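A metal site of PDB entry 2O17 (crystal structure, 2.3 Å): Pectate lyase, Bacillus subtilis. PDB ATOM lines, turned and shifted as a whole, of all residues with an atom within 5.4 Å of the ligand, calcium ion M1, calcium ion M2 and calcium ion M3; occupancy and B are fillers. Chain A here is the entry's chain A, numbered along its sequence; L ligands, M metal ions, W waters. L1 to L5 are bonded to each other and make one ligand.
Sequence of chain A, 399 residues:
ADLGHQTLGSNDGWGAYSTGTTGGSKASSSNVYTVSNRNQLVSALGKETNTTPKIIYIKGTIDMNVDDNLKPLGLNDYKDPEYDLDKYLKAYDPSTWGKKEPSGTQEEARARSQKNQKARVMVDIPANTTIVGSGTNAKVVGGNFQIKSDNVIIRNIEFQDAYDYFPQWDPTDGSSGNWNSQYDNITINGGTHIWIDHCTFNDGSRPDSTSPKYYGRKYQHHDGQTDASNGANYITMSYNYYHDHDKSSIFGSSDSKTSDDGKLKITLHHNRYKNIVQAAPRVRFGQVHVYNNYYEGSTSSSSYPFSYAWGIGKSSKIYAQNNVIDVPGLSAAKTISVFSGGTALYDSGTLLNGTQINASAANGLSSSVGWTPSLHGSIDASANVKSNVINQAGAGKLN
An oxygen (O6) of LG4 L4 is in salt-bridge range of the side-chain amino group of Lys 257, at 3.0 Å. NZ of Lys 247 lies close to O6 of LG2 L2, 2.8 Å away. The side-chain amide nitrogen (ND2) of Asn 230 sits at hydrogen-bond distance from an oxygen (O1) of LG5 L5, 3.0 Å away. The side-chain amide nitrogen (ND2) of Asn 178 is in hydrogen-bond range of an oxygen (O2) of LIG L1 (3.5 Å). The side-chain amide oxygen (OE1) of Gln 278 sits close to an oxygen (O5) of LIG L1, 3.4 Å away. An oxygen (O5) of LG5 L5 is in salt-bridge range of the side-chain amino group (NZ) of Lys 118, 3.5 Å away. An oxygen (O6) of LG4 L4 is in hydrogen-bond range of the side-chain hydroxyl (OG) of Ser 253, 2.7 Å away. O7 of LIG L1 lies within salt-bridge range of NE of Arg 282, at 2.8 Å. OE1 of Gln 182 is in hydrogen-bond range of O1 of LG4 L4 (3.1 Å). An oxygen (O2) of LG5 L5 lies within hydrogen-bond range of the side-chain amide nitrogen of Asn 189, at 2.6 Å. The guanidinium group (NH1) of Arg 284 sits at hydrogen-bond distance from an oxygen (O2) of LG2 L2, 2.9 Å away.
The side-chain hydroxyl (OG) of Ser 229 lies within hydrogen-bond range of the side-chain hydroxyl (OG) of Ser 253, 3.1 Å away. The backbone carbonyl oxygen (O) of Asp 173 sits at hydrogen-bond distance from the side-chain amide nitrogen (ND2) of Asn 178 (3.1 Å). The backbone NH of Ile 250 lies within hydrogen-bond range of the side-chain carboxylate of Asp 227 (2.9 Å). OE1 of Gln 146 is in hydrogen-bond range of ND2 of Asn 189 (3.1 Å). OD2 of Asp 184 lies close to OG1 of Thr 187. The guanidinium group of Arg 284 is in hydrogen-bond range of the backbone carbonyl oxygen of Gly 252. The side-chain carboxylate (OD1) of Asp 184 sits close to the backbone NH (N) of Gly 224. The side-chain amide nitrogen (ND2) of Asn 230 sits at hydrogen-bond distance from the side-chain amide oxygen (OD1) of Asn 189, at 2.9 Å.
Residues that only touch the ligand: Ile 250 (3.5 Å), Phe 339 (3.8 Å) and Ser 229 (3.9 Å). Hydrophobic or aromatic side chains within 4 Å of the ligand: Ile 250 and Phe 339.
Within 4 Å of calcium ion M1: Asp 184, Asp 223 and Asp 227. The nearest printed residue that does not touch calcium ion M1 is Gly 224 (4.4 Å).
The nearest printed residue that does not touch calcium ion M2 is Lys 247 (4.4 Å).
One residue has an atom within 4 Å of calcium ion M3: Asp 223.
Calcium ion M1 is bound by OD2 of Asp 227 (2.3 Å), OD1 of Asp 184 (2.3 Å), OD2 of Asp 223 (2.3 Å), OD2 of Asp 184 (2.5 Å), water W8 (2.6 Å), O6 of LG3 L3 (2.6 Å) and water W9 (2.8 Å). Calcium ion M1 has seven donor atoms within binding distance.
Calcium ion M2 is bound by an oxygen (O6) of LG2 L2 (2.3 Å), the side-chain amide oxygen of Asn 180 (2.4 Å), the side-chain carboxylate of Asp 173 (2.5 Å), water W6 (2.5 Å), water W1 (2.6 Å), an oxygen (O3) of LIG L1 (2.7 Å) and an oxygen (O4) of LG2 L2 (2.7 Å). Calcium ion M2 has seven donor atoms within binding distance.
Calcium ion M3 is bound by OD1 of Asp 223 (2.3 Å), O4 of LG3 L3 (2.3 Å), O6 of LG3 L3 (2.3 Å), water W19 (2.5 Å), O5 of LG2 L2 (2.6 Å), water W4 (2.6 Å), water W10 (2.7 Å) and OD2 of Asp 223 (2.8 Å). Calcium ion M3 has eight donor atoms within binding distance.
Water W9 lies within hydrogen-bond range of the backbone carbonyl oxygen (O) of Gln 182 (2.6 Å) and an oxygen (O1) of LG4 L4 (3.0 Å). Water W6 bridges an oxygen (O2) of LIG L1 (2.7 Å) and the side-chain amino group (NZ) of Lys 247 (3.5 Å). Water W10 lies within hydrogen-bond range of O1 of LG4 L4 (2.6 Å) and O of Ser 181 (3.1 Å). Water W14 lies within hydrogen-bond range of an oxygen (O4) of LG4 L4 (2.6 Å), the side-chain hydroxyl (OG) of Ser 229 (2.8 Å) and the side-chain amide nitrogen (ND2) of Asn 230 (3.4 Å). Water W18 lies within hydrogen-bond range of OH of Tyr 308, OE1 of Gln 278 and O7 of LIG L1. Water W17 bridges an oxygen (O5) of LG3 L3 (2.7 Å) and the backbone carbonyl oxygen (O) of Ile 250 (3.1 Å).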
ATOM      1  N   LYS A 118     -26.635 -22.760 -32.319  1.00  0.00           N
ATOM      2  CA  LYS A 118     -27.478 -22.783 -31.123  1.00  0.00           C
ATOM      3  C   LYS A 118     -28.020 -24.177 -30.855  1.00  0.00           C
ATOM      4  O   LYS A 118     -28.073 -24.623 -29.696  1.00  0.00           O
ATOM      5  CB  LYS A 118     -28.628 -21.783 -31.307  1.00  0.00           C
ATOM      6  CG  LYS A 118     -29.732 -21.887 -30.294  1.00  0.00           C
ATOM      7  CD  LYS A 118     -30.986 -21.175 -30.785  1.00  0.00           C
ATOM      8  CE  LYS A 118     -32.074 -21.328 -29.747  1.00  0.00           C
ATOM      9  NZ  LYS A 118     -32.676 -19.994 -29.446  1.00  0.00           N
ATOM     10  N   GLN A 146     -29.253 -24.116 -20.207  1.00  0.00           N
ATOM     11  CA  GLN A 146     -30.420 -23.238 -19.920  1.00  0.00           C
ATOM     12  C   GLN A 146     -31.357 -23.866 -18.903  1.00  0.00           C
ATOM     13  O   GLN A 146     -31.731 -25.032 -19.021  1.00  0.00           O
ATOM     14  CB  GLN A 146     -31.200 -22.832 -21.198  1.00  0.00           C
ATOM     15  CG  GLN A 146     -32.454 -21.978 -20.920  1.00  0.00           C
ATOM     16  CD  GLN A 146     -33.103 -21.408 -22.180  1.00  0.00           C
ATOM     17  OE1 GLN A 146     -33.112 -20.195 -22.389  1.00  0.00           O
ATOM     18  NE2 GLN A 146     -33.669 -22.276 -23.012  1.00  0.00           N
ATOM     19  N   ASP A 173     -26.157   0.564 -30.166  1.00  0.00           N
ATOM     20  CA  ASP A 173     -25.788   0.032 -28.844  1.00  0.00           C
ATOM     21  C   ASP A 173     -24.637   0.844 -28.255  1.00  0.00           C
ATOM     22  O   ASP A 173     -23.453   0.603 -28.522  1.00  0.00           O
ATOM     23  CB  ASP A 173     -25.421  -1.458 -28.920  1.00  0.00           C
ATOM     24  CG  ASP A 173     -25.227  -2.092 -27.541  1.00  0.00           C
ATOM     25  OD1 ASP A 173     -25.285  -1.374 -26.513  1.00  0.00           O
ATOM     26  OD2 ASP A 173     -25.008  -3.322 -27.491  1.00  0.00           O
ATOM     27  N   GLY A 174     -25.007   1.824 -27.435  1.00  0.00           N
ATOM     28  CA  GLY A 174     -24.054   2.814 -26.978  1.00  0.00           C
ATOM     29  C   GLY A 174     -23.758   3.797 -28.101  1.00  0.00           C
ATOM     30  O   GLY A 174     -24.361   3.727 -29.179  1.00  0.00           O
ATOM     31  N   ASN A 178     -22.004  -1.630 -30.833  1.00  0.00           N
ATOM     32  CA  ASN A 178     -21.357  -2.776 -30.188  1.00  0.00           C
ATOM     33  C   ASN A 178     -21.730  -4.025 -30.942  1.00  0.00           C
ATOM     34  O   ASN A 178     -22.778  -4.067 -31.576  1.00  0.00           O
ATOM     35  CB  ASN A 178     -21.797  -2.951 -28.728  1.00  0.00           C
ATOM     36  CG  ASN A 178     -20.954  -2.143 -27.760  1.00  0.00           C
ATOM     37  OD1 ASN A 178     -19.736  -2.262 -27.720  1.00  0.00           O
ATOM     38  ND2 ASN A 178     -21.618  -1.313 -26.959  1.00  0.00           N
ATOM     39  N   ASN A 180     -22.868  -7.879 -30.260  1.00  0.00           N
ATOM     40  CA  ASN A 180     -23.494  -8.700 -29.214  1.00  0.00           C
ATOM     41  C   ASN A 180     -23.664 -10.171 -29.592  1.00  0.00           C
ATOM     42  O   ASN A 180     -24.089 -10.485 -30.709  1.00  0.00           O
ATOM     43  CB  ASN A 180     -24.870  -8.152 -28.839  1.00  0.00           C
ATOM     44  CG  ASN A 180     -24.814  -6.767 -28.269  1.00  0.00           C
ATOM     45  OD1 ASN A 180     -24.465  -6.571 -27.101  1.00  0.00           O
ATOM     46  ND2 ASN A 180     -25.160  -5.769 -29.097  1.00  0.00           N
ATOM     47  N   SER A 181     -23.362 -11.062 -28.648  1.00  0.00           N
ATOM     48  CA  SER A 181     -23.504 -12.494 -28.886  1.00  0.00           C
ATOM     49  C   SER A 181     -24.549 -13.116 -27.943  1.00  0.00           C
ATOM     50  O   SER A 181     -25.066 -12.429 -27.055  1.00  0.00           O
ATOM     51  CB  SER A 181     -22.127 -13.171 -28.759  1.00  0.00           C
ATOM     52  OG  SER A 181     -21.324 -12.848 -29.898  1.00  0.00           O
ATOM     53  N   GLN A 182     -24.853 -14.398 -28.157  1.00  0.00           N
ATOM     54  CA  GLN A 182     -25.990 -15.049 -27.499  1.00  0.00           C
ATOM     55  C   GLN A 182     -25.712 -16.021 -26.329  1.00  0.00           C
ATOM     56  O   GLN A 182     -26.539 -16.137 -25.421  1.00  0.00           O
ATOM     57  CB  GLN A 182     -26.884 -15.755 -28.538  1.00  0.00           C
ATOM     58  CG  GLN A 182     -27.605 -14.822 -29.543  1.00  0.00           C
ATOM     59  CD  GLN A 182     -28.446 -13.736 -28.872  1.00  0.00           C
ATOM     60  OE1 GLN A 182     -29.393 -14.018 -28.123  1.00  0.00           O
ATOM     61  NE2 GLN A 182     -28.100 -12.491 -29.137  1.00  0.00           N
ATOM     62  N   ASP A 184     -24.422 -17.708 -22.961  1.00  0.00           N
ATOM     63  CA  ASP A 184     -23.866 -17.685 -21.604  1.00  0.00           C
ATOM     64  C   ASP A 184     -23.356 -19.085 -21.255  1.00  0.00           C
ATOM     65  O   ASP A 184     -23.654 -20.034 -21.961  1.00  0.00           O
ATOM     66  CB  ASP A 184     -24.943 -17.297 -20.576  1.00  0.00           C
ATOM     67  CG  ASP A 184     -25.790 -16.123 -21.013  1.00  0.00           C
ATOM     68  OD1 ASP A 184     -25.217 -15.098 -21.467  1.00  0.00           O
ATOM     69  OD2 ASP A 184     -27.038 -16.227 -20.888  1.00  0.00           O
ATOM     70  N   THR A 187     -27.751 -19.868 -18.456  1.00  0.00           N
ATOM     71  CA  THR A 187     -28.854 -18.906 -18.553  1.00  0.00           C
ATOM     72  C   THR A 187     -29.998 -19.452 -17.708  1.00  0.00           C
ATOM     73  O   THR A 187     -30.465 -20.553 -17.952  1.00  0.00           O
ATOM     74  CB  THR A 187     -29.397 -18.768 -20.016  1.00  0.00           C
ATOM     75  OG1 THR A 187     -28.306 -18.562 -20.944  1.00  0.00           O
ATOM     76  CG2 THR A 187     -30.408 -17.606 -20.105  1.00  0.00           C
ATOM     77  N   ASN A 189     -33.583 -18.911 -17.294  1.00  0.00           N
ATOM     78  CA  ASN A 189     -34.674 -18.290 -18.036  1.00  0.00           C
ATOM     79  C   ASN A 189     -36.043 -18.639 -17.416  1.00  0.00           C
ATOM     80  O   ASN A 189     -36.726 -19.550 -17.887  1.00  0.00           O
ATOM     81  CB  ASN A 189     -34.605 -18.730 -19.501  1.00  0.00           C
ATOM     82  CG  ASN A 189     -35.474 -17.882 -20.416  1.00  0.00           C
ATOM     83  OD1 ASN A 189     -36.203 -16.983 -19.986  1.00  0.00           O
ATOM     84  ND2 ASN A 189     -35.401 -18.185 -21.715  1.00  0.00           N
ATOM     85  N   ASP A 223     -21.028 -13.816 -24.263  1.00  0.00           N
ATOM     86  CA  ASP A 223     -22.071 -13.065 -23.602  1.00  0.00           C
ATOM     87  C   ASP A 223     -21.839 -13.144 -22.104  1.00  0.00           C
ATOM     88  O   ASP A 223     -20.790 -12.693 -21.635  1.00  0.00           O
ATOM     89  CB  ASP A 223     -23.461 -13.554 -24.005  1.00  0.00           C
ATOM     90  CG  ASP A 223     -24.550 -12.540 -23.685  1.00  0.00           C
ATOM     91  OD1 ASP A 223     -24.365 -11.352 -24.036  1.00  0.00           O
ATOM     92  OD2 ASP A 223     -25.580 -12.928 -23.078  1.00  0.00           O
ATOM     93  N   GLY A 224     -22.785 -13.719 -21.371  1.00  0.00           N
ATOM     94  CA  GLY A 224     -22.699 -13.786 -19.906  1.00  0.00           C
ATOM     95  C   GLY A 224     -22.021 -15.051 -19.384  1.00  0.00           C
ATOM     96  O   GLY A 224     -21.634 -15.932 -20.150  1.00  0.00           O
ATOM     97  N   ASP A 227     -26.237 -15.551 -16.162  1.00  0.00           N
ATOM     98  CA  ASP A 227     -27.336 -14.597 -16.316  1.00  0.00           C
ATOM     99  C   ASP A 227     -28.658 -15.174 -15.777  1.00  0.00           C
ATOM    100  O   ASP A 227     -28.885 -16.391 -15.825  1.00  0.00           O
ATOM    101  CB  ASP A 227     -27.513 -14.241 -17.800  1.00  0.00           C
ATOM    102  CG  ASP A 227     -26.450 -13.292 -18.319  1.00  0.00           C
ATOM    103  OD1 ASP A 227     -25.673 -12.772 -17.502  1.00  0.00           O
ATOM    104  OD2 ASP A 227     -26.400 -13.043 -19.540  1.00  0.00           O
ATOM    105  N   SER A 229     -33.018 -14.153 -15.824  1.00  0.00           N
ATOM    106  CA  SER A 229     -33.918 -13.406 -16.698  1.00  0.00           C
ATOM    107  C   SER A 229     -35.354 -13.879 -16.520  1.00  0.00           C
ATOM    108  O   SER A 229     -35.588 -14.981 -16.007  1.00  0.00           O
ATOM    109  CB  SER A 229     -33.498 -13.696 -18.149  1.00  0.00           C
ATOM    110  OG  SER A 229     -33.945 -12.678 -19.034  1.00  0.00           O
ATOM    111  N   ASN A 230     -36.304 -13.046 -16.960  1.00  0.00           N
ATOM    112  CA  ASN A 230     -37.729 -13.427 -17.091  1.00  0.00           C
ATOM    113  C   ASN A 230     -38.365 -14.133 -15.899  1.00  0.00           C
ATOM    114  O   ASN A 230     -38.918 -15.226 -16.028  1.00  0.00           O
ATOM    115  CB  ASN A 230     -37.982 -14.269 -18.358  1.00  0.00           C
ATOM    116  CG  ASN A 230     -37.607 -13.529 -19.641  1.00  0.00           C
ATOM    117  OD1 ASN A 230     -37.920 -12.338 -19.806  1.00  0.00           O
ATOM    118  ND2 ASN A 230     -36.919 -14.221 -20.534  1.00  0.00           N
ATOM    119  N   LYS A 247     -18.563  -9.292 -19.498  1.00  0.00           N
ATOM    120  CA  LYS A 247     -19.841  -9.158 -18.774  1.00  0.00           C
ATOM    121  C   LYS A 247     -20.232 -10.455 -18.077  1.00  0.00           C
ATOM    122  O   LYS A 247     -20.565 -11.451 -18.741  1.00  0.00           O
ATOM    123  CB  LYS A 247     -20.977  -8.702 -19.720  1.00  0.00           C
ATOM    124  CG  LYS A 247     -20.634  -7.481 -20.596  1.00  0.00           C
ATOM    125  CD  LYS A 247     -21.642  -7.243 -21.763  1.00  0.00           C
ATOM    126  CE  LYS A 247     -21.462  -8.272 -22.919  1.00  0.00           C
ATOM    127  NZ  LYS A 247     -21.975  -7.786 -24.265  1.00  0.00           N
ATOM    128  N   ILE A 250     -25.766 -10.680 -15.472  1.00  0.00           N
ATOM    129  CA  ILE A 250     -26.858  -9.745 -15.633  1.00  0.00           C
ATOM    130  C   ILE A 250     -28.167 -10.359 -15.120  1.00  0.00           C
ATOM    131  O   ILE A 250     -28.664 -11.347 -15.679  1.00  0.00           O
ATOM    132  CB  ILE A 250     -26.969  -9.244 -17.103  1.00  0.00           C
ATOM    133  CG1 ILE A 250     -25.684  -8.488 -17.462  1.00  0.00           C
ATOM    134  CG2 ILE A 250     -28.263  -8.399 -17.325  1.00  0.00           C
ATOM    135  CD1 ILE A 250     -25.644  -7.883 -18.849  1.00  0.00           C
ATOM    136  N   GLY A 252     -31.968  -9.768 -14.621  1.00  0.00           N
ATOM    137  CA  GLY A 252     -33.000  -8.897 -15.163  1.00  0.00           C
ATOM    138  C   GLY A 252     -32.531  -8.250 -16.453  1.00  0.00           C
ATOM    139  O   GLY A 252     -31.669  -7.361 -16.452  1.00  0.00           O
ATOM    140  N   SER A 253     -33.095  -8.703 -17.557  1.00  0.00           N
ATOM    141  CA  SER A 253     -32.583  -8.374 -18.879  1.00  0.00           C
ATOM    142  C   SER A 253     -33.107  -7.070 -19.509  1.00  0.00           C
ATOM    143  O   SER A 253     -32.589  -6.630 -20.532  1.00  0.00           O
ATOM    144  CB  SER A 253     -32.822  -9.559 -19.830  1.00  0.00           C
ATOM    145  OG  SER A 253     -34.201  -9.779 -20.053  1.00  0.00           O
ATOM    146  N   SER A 254     -34.113  -6.442 -18.885  1.00  0.00           N
ATOM    147  CA  SER A 254     -34.798  -5.316 -19.532  1.00  0.00           C
ATOM    148  C   SER A 254     -35.499  -4.386 -18.529  1.00  0.00           C
ATOM    149  O   SER A 254     -36.202  -4.865 -17.630  1.00  0.00           O
ATOM    150  CB  SER A 254     -35.785  -5.851 -20.586  1.00  0.00           C
ATOM    151  OG  SER A 254     -36.614  -4.826 -21.128  1.00  0.00           O
ATOM    152  N   LYS A 257     -39.287  -5.135 -18.354  1.00  0.00           N
ATOM    153  CA  LYS A 257     -39.801  -6.342 -17.731  1.00  0.00           C
ATOM    154  C   LYS A 257     -40.131  -6.069 -16.266  1.00  0.00           C
ATOM    155  O   LYS A 257     -39.511  -6.628 -15.355  1.00  0.00           O
ATOM    156  CB  LYS A 257     -38.833  -7.513 -17.923  1.00  0.00           C
ATOM    157  CG  LYS A 257     -39.201  -8.445 -19.077  1.00  0.00           C
ATOM    158  CD  LYS A 257     -38.040  -8.673 -20.039  1.00  0.00           C
ATOM    159  CE  LYS A 257     -38.496  -9.328 -21.347  1.00  0.00           C
ATOM    160  NZ  LYS A 257     -37.955 -10.720 -21.559  1.00  0.00           N
ATOM    161  N   GLN A 278     -17.064  -6.060 -15.852  1.00  0.00           N
ATOM    162  CA  GLN A 278     -18.283  -5.401 -15.391  1.00  0.00           C
ATOM    163  C   GLN A 278     -19.367  -6.409 -15.019  1.00  0.00           C
ATOM    164  O   GLN A 278     -19.222  -7.614 -15.272  1.00  0.00           O
ATOM    165  CB  GLN A 278     -18.811  -4.454 -16.479  1.00  0.00           C
ATOM    166  CG  GLN A 278     -19.191  -5.144 -17.804  1.00  0.00           C
ATOM    167  CD  GLN A 278     -19.456  -4.146 -18.928  1.00  0.00           C
ATOM    168  OE1 GLN A 278     -20.361  -3.306 -18.847  1.00  0.00           O
ATOM    169  NE2 GLN A 278     -18.668  -4.244 -19.996  1.00  0.00           N
ATOM    170  N   ARG A 282     -24.838  -7.086 -12.369  1.00  0.00           N
ATOM    171  CA  ARG A 282     -25.714  -5.979 -12.773  1.00  0.00           C
ATOM    172  C   ARG A 282     -27.171  -6.360 -12.504  1.00  0.00           C
ATOM    173  O   ARG A 282     -27.657  -7.361 -13.034  1.00  0.00           O
ATOM    174  CB  ARG A 282     -25.516  -5.659 -14.263  1.00  0.00           C
ATOM    175  CG  ARG A 282     -26.195  -4.367 -14.741  1.00  0.00           C
ATOM    176  CD  ARG A 282     -26.727  -4.526 -16.176  1.00  0.00           C
ATOM    177  NE  ARG A 282     -27.025  -3.225 -16.783  1.00  0.00           N
ATOM    178  CZ  ARG A 282     -28.135  -2.511 -16.570  1.00  0.00           C
ATOM    179  NH1 ARG A 282     -29.119  -2.957 -15.775  1.00  0.00           N
ATOM    180  NH2 ARG A 282     -28.266  -1.348 -17.174  1.00  0.00           N
ATOM    181  N   ARG A 284     -31.412  -5.478 -12.105  1.00  0.00           N
ATOM    182  CA  ARG A 284     -32.656  -4.739 -12.246  1.00  0.00           C
ATOM    183  C   ARG A 284     -33.674  -5.402 -11.317  1.00  0.00           C
ATOM    184  O   ARG A 284     -33.721  -6.643 -11.235  1.00  0.00           O
ATOM    185  CB  ARG A 284     -33.196  -4.821 -13.681  1.00  0.00           C
ATOM    186  CG  ARG A 284     -32.486  -3.961 -14.681  1.00  0.00           C
ATOM    187  CD  ARG A 284     -32.919  -4.328 -16.105  1.00  0.00           C
ATOM    188  NE  ARG A 284     -32.233  -3.507 -17.102  1.00  0.00           N
ATOM    189  CZ  ARG A 284     -31.214  -3.906 -17.867  1.00  0.00           C
ATOM    190  NH1 ARG A 284     -30.734  -5.148 -17.794  1.00  0.00           N
ATOM    191  NH2 ARG A 284     -30.678  -3.046 -18.722  1.00  0.00           N
ATOM    192  N   TYR A 308     -16.581  -1.795 -13.432  1.00  0.00           N
ATOM    193  CA  TYR A 308     -17.265  -1.756 -12.126  1.00  0.00           C
ATOM    194  C   TYR A 308     -17.565  -3.147 -11.579  1.00  0.00           C
ATOM    195  O   TYR A 308     -17.420  -4.153 -12.282  1.00  0.00           O
ATOM    196  CB  TYR A 308     -18.563  -0.907 -12.193  1.00  0.00           C
ATOM    197  CG  TYR A 308     -19.698  -1.569 -12.935  1.00  0.00           C
ATOM    198  CD1 TYR A 308     -20.581  -2.432 -12.273  1.00  0.00           C
ATOM    199  CD2 TYR A 308     -19.881  -1.372 -14.301  1.00  0.00           C
ATOM    200  CE1 TYR A 308     -21.612  -3.059 -12.945  1.00  0.00           C
ATOM    201  CE2 TYR A 308     -20.925  -1.980 -14.978  1.00  0.00           C
ATOM    202  CZ  TYR A 308     -21.787  -2.830 -14.297  1.00  0.00           C
ATOM    203  OH  TYR A 308     -22.818  -3.443 -14.963  1.00  0.00           O
ATOM    204  N   PHE A 339     -27.310   3.192 -12.828  1.00  0.00           N
ATOM    205  CA  PHE A 339     -28.096   3.374 -14.049  1.00  0.00           C
ATOM    206  C   PHE A 339     -29.414   4.026 -13.689  1.00  0.00           C
ATOM    207  O   PHE A 339     -29.821   4.005 -12.520  1.00  0.00           O
ATOM    208  CB  PHE A 339     -28.311   2.017 -14.743  1.00  0.00           C
ATOM    209  CG  PHE A 339     -27.026   1.317 -15.095  1.00  0.00           C
ATOM    210  CD1 PHE A 339     -26.364   1.606 -16.285  1.00  0.00           C
ATOM    211  CD2 PHE A 339     -26.458   0.392 -14.223  1.00  0.00           C
ATOM    212  CE1 PHE A 339     -25.159   0.994 -16.619  1.00  0.00           C
ATOM    213  CE2 PHE A 339     -25.257  -0.246 -14.535  1.00  0.00           C
ATOM    214  CZ  PHE A 339     -24.600   0.068 -15.727  1.00  0.00           C
HETATM  215  C1  LIG L   1     -22.136  -2.039 -21.420  1.00  0.00           C
HETATM  216  C2  LIG L   1     -22.722  -2.596 -22.712  1.00  0.00           C
HETATM  217  C3  LIG L   1     -23.930  -1.777 -23.131  1.00  0.00           C
HETATM  218  C4  LIG L   1     -24.961  -1.707 -21.993  1.00  0.00           C
HETATM  219  C5  LIG L   1     -24.338  -1.417 -20.602  1.00  0.00           C
HETATM  220  C6  LIG L   1     -25.313  -1.675 -19.476  1.00  0.00           C
HETATM  221  O1  LIG L   1     -21.766  -0.648 -21.577  1.00  0.00           O
HETATM  222  O2  LIG L   1     -21.760  -2.643 -23.772  1.00  0.00           O
HETATM  223  O3  LIG L   1     -24.477  -2.413 -24.278  1.00  0.00           O
HETATM  224  O4  LIG L   1     -25.710  -2.927 -21.913  1.00  0.00           O
HETATM  225  O5  LIG L   1     -23.130  -2.182 -20.400  1.00  0.00           O
HETATM  226  O6  LIG L   1     -26.436  -1.133 -19.523  1.00  0.00           O
HETATM  227  O7  LIG L   1     -24.965  -2.409 -18.526  1.00  0.00           O
HETATM  228  C1  LG2 L   2     -26.882  -3.567 -22.432  1.00  0.00           C
HETATM  229  C2  LG2 L   2     -28.087  -3.937 -21.564  1.00  0.00           C
HETATM  230  C3  LG2 L   2     -27.783  -5.149 -20.679  1.00  0.00           C
HETATM  231  C4  LG2 L   2     -27.138  -6.261 -21.503  1.00  0.00           C
HETATM  232  C5  LG2 L   2     -25.896  -5.729 -22.233  1.00  0.00           C
HETATM  233  C6  LG2 L   2     -25.137  -6.810 -22.944  1.00  0.00           C
HETATM  234  O1  LG2 L   2     -28.459  -2.808 -20.768  1.00  0.00           O
HETATM  235  O2  LG2 L   2     -28.990  -5.648 -20.083  1.00  0.00           O
HETATM  236  O3  LG2 L   2     -28.094  -6.754 -22.459  1.00  0.00           O
HETATM  237  O4  LG2 L   2     -26.320  -4.690 -23.117  1.00  0.00           O
HETATM  238  O5  LG2 L   2     -25.182  -7.954 -22.440  1.00  0.00           O
HETATM  239  O6  LG2 L   2     -24.508  -6.540 -23.995  1.00  0.00           O
HETATM  240  C1  LG3 L   3     -28.263  -7.648 -23.576  1.00  0.00           C
HETATM  241  C2  LG3 L   3     -29.525  -7.532 -24.418  1.00  0.00           C
HETATM  242  C3  LG3 L   3     -30.732  -7.953 -23.571  1.00  0.00           C
HETATM  243  C4  LG3 L   3     -30.508  -9.330 -22.906  1.00  0.00           C
HETATM  244  C5  LG3 L   3     -29.177  -9.378 -22.159  1.00  0.00           C
HETATM  245  C6  LG3 L   3     -28.890 -10.769 -21.667  1.00  0.00           C
HETATM  246  O1  LG3 L   3     -29.648  -6.183 -24.865  1.00  0.00           O
HETATM  247  O2  LG3 L   3     -31.925  -7.911 -24.371  1.00  0.00           O
HETATM  248  O3  LG3 L   3     -30.552 -10.393 -23.872  1.00  0.00           O
HETATM  249  O4  LG3 L   3     -28.125  -8.981 -23.043  1.00  0.00           O
HETATM  250  O5  LG3 L   3     -29.635 -11.267 -20.791  1.00  0.00           O
HETATM  251  O6  LG3 L   3     -27.908 -11.389 -22.160  1.00  0.00           O
HETATM  252  C1  LG4 L   4     -31.248 -11.650 -23.694  1.00  0.00           C
HETATM  253  C2  LG4 L   4     -31.181 -12.372 -25.038  1.00  0.00           C
HETATM  254  C3  LG4 L   4     -32.097 -11.717 -26.073  1.00  0.00           C
HETATM  255  C4  LG4 L   4     -33.489 -11.397 -25.523  1.00  0.00           C
HETATM  256  C5  LG4 L   4     -33.425 -10.765 -24.126  1.00  0.00           C
HETATM  257  C6  LG4 L   4     -34.790 -10.494 -23.517  1.00  0.00           C
HETATM  258  O1  LG4 L   4     -29.835 -12.375 -25.514  1.00  0.00           O
HETATM  259  O2  LG4 L   4     -32.182 -12.565 -27.215  1.00  0.00           O
HETATM  260  O3  LG4 L   4     -34.285 -12.586 -25.458  1.00  0.00           O
HETATM  261  O4  LG4 L   4     -32.607 -11.563 -23.249  1.00  0.00           O
HETATM  262  O5  LG4 L   4     -35.606  -9.803 -24.177  1.00  0.00           O
HETATM  263  O6  LG4 L   4     -35.055 -10.950 -22.386  1.00  0.00           O
HETATM  264  C1  LG5 L   5     -35.490 -13.319 -25.649  1.00  0.00           C
HETATM  265  C2  LG5 L   5     -36.049 -14.236 -24.548  1.00  0.00           C
HETATM  266  C3  LG5 L   5     -35.195 -15.494 -24.363  1.00  0.00           C
HETATM  267  C4  LG5 L   5     -34.857 -16.188 -25.689  1.00  0.00           C
HETATM  268  C5  LG5 L   5     -34.366 -15.192 -26.753  1.00  0.00           C
HETATM  269  C6  LG5 L   5     -34.290 -15.816 -28.110  1.00  0.00           C
HETATM  270  O1  LG5 L   5     -36.114 -13.504 -23.318  1.00  0.00           O
HETATM  271  O2  LG5 L   5     -35.917 -16.399 -23.527  1.00  0.00           O
HETATM  272  O3  LG5 L   5     -36.001 -16.900 -26.169  1.00  0.00           O
HETATM  273  O4  LG5 L   5     -35.243 -14.055 -26.849  1.00  0.00           O
HETATM  274  O5  LG5 L   5     -34.153 -17.065 -28.207  1.00  0.00           O
HETATM  275  O6  LG5 L   5     -34.378 -15.060 -29.099  1.00  0.00           O
HETATM  276 CA    CA M   1     -27.148 -13.814 -21.594  1.00  0.00          CA
HETATM  277 CA    CA M   2     -24.961  -4.819 -25.500  1.00  0.00          CA
HETATM  278 CA    CA M   3     -26.165 -10.218 -23.154  1.00  0.00          CA
HETATM  279  O   HOH W   1     -27.451  -4.730 -26.128  1.00  0.00           O
HETATM  280  O   HOH W   2     -18.811  -1.408 -22.502  1.00  0.00           O
HETATM  281  O   HOH W   3     -35.213  -8.557 -26.379  1.00  0.00           O
HETATM  282  O   HOH W   4     -25.923  -9.108 -25.474  1.00  0.00           O
HETATM  283  O   HOH W   5     -22.183   0.736 -19.337  1.00  0.00           O
HETATM  284  O   HOH W   6     -22.437  -4.589 -25.551  1.00  0.00           O
HETATM  285  O   HOH W   7     -20.743   0.534 -24.534  1.00  0.00           O
HETATM  286  O   HOH W   8     -29.557 -13.946 -20.649  1.00  0.00           O
HETATM  287  O   HOH W   9     -28.030 -14.340 -24.248  1.00  0.00           O
HETATM  288  O   HOH W  10     -27.357 -11.518 -25.208  1.00  0.00           O
HETATM  289  O   HOH W  11     -35.824 -19.295 -27.477  1.00  0.00           O
HETATM  290  O   HOH W  12     -37.828 -13.979 -28.267  1.00  0.00           O
HETATM  291  O   HOH W  13     -31.080  -4.163 -23.678  1.00  0.00           O
HETATM  292  O   HOH W  14     -33.891 -13.311 -21.739  1.00  0.00           O
HETATM  293  O   HOH W  15     -26.788   1.330 -20.812  1.00  0.00           O
HETATM  294  O   HOH W  16     -18.488  -3.828 -24.056  1.00  0.00           O
HETATM  295  O   HOH W  17     -30.401 -11.756 -18.202  1.00  0.00           O
HETATM  296  O   HOH W  18     -22.668  -3.329 -17.571  1.00  0.00           O
HETATM  297  O   HOH W  19     -25.086 -10.684 -20.953  1.00  0.00           O
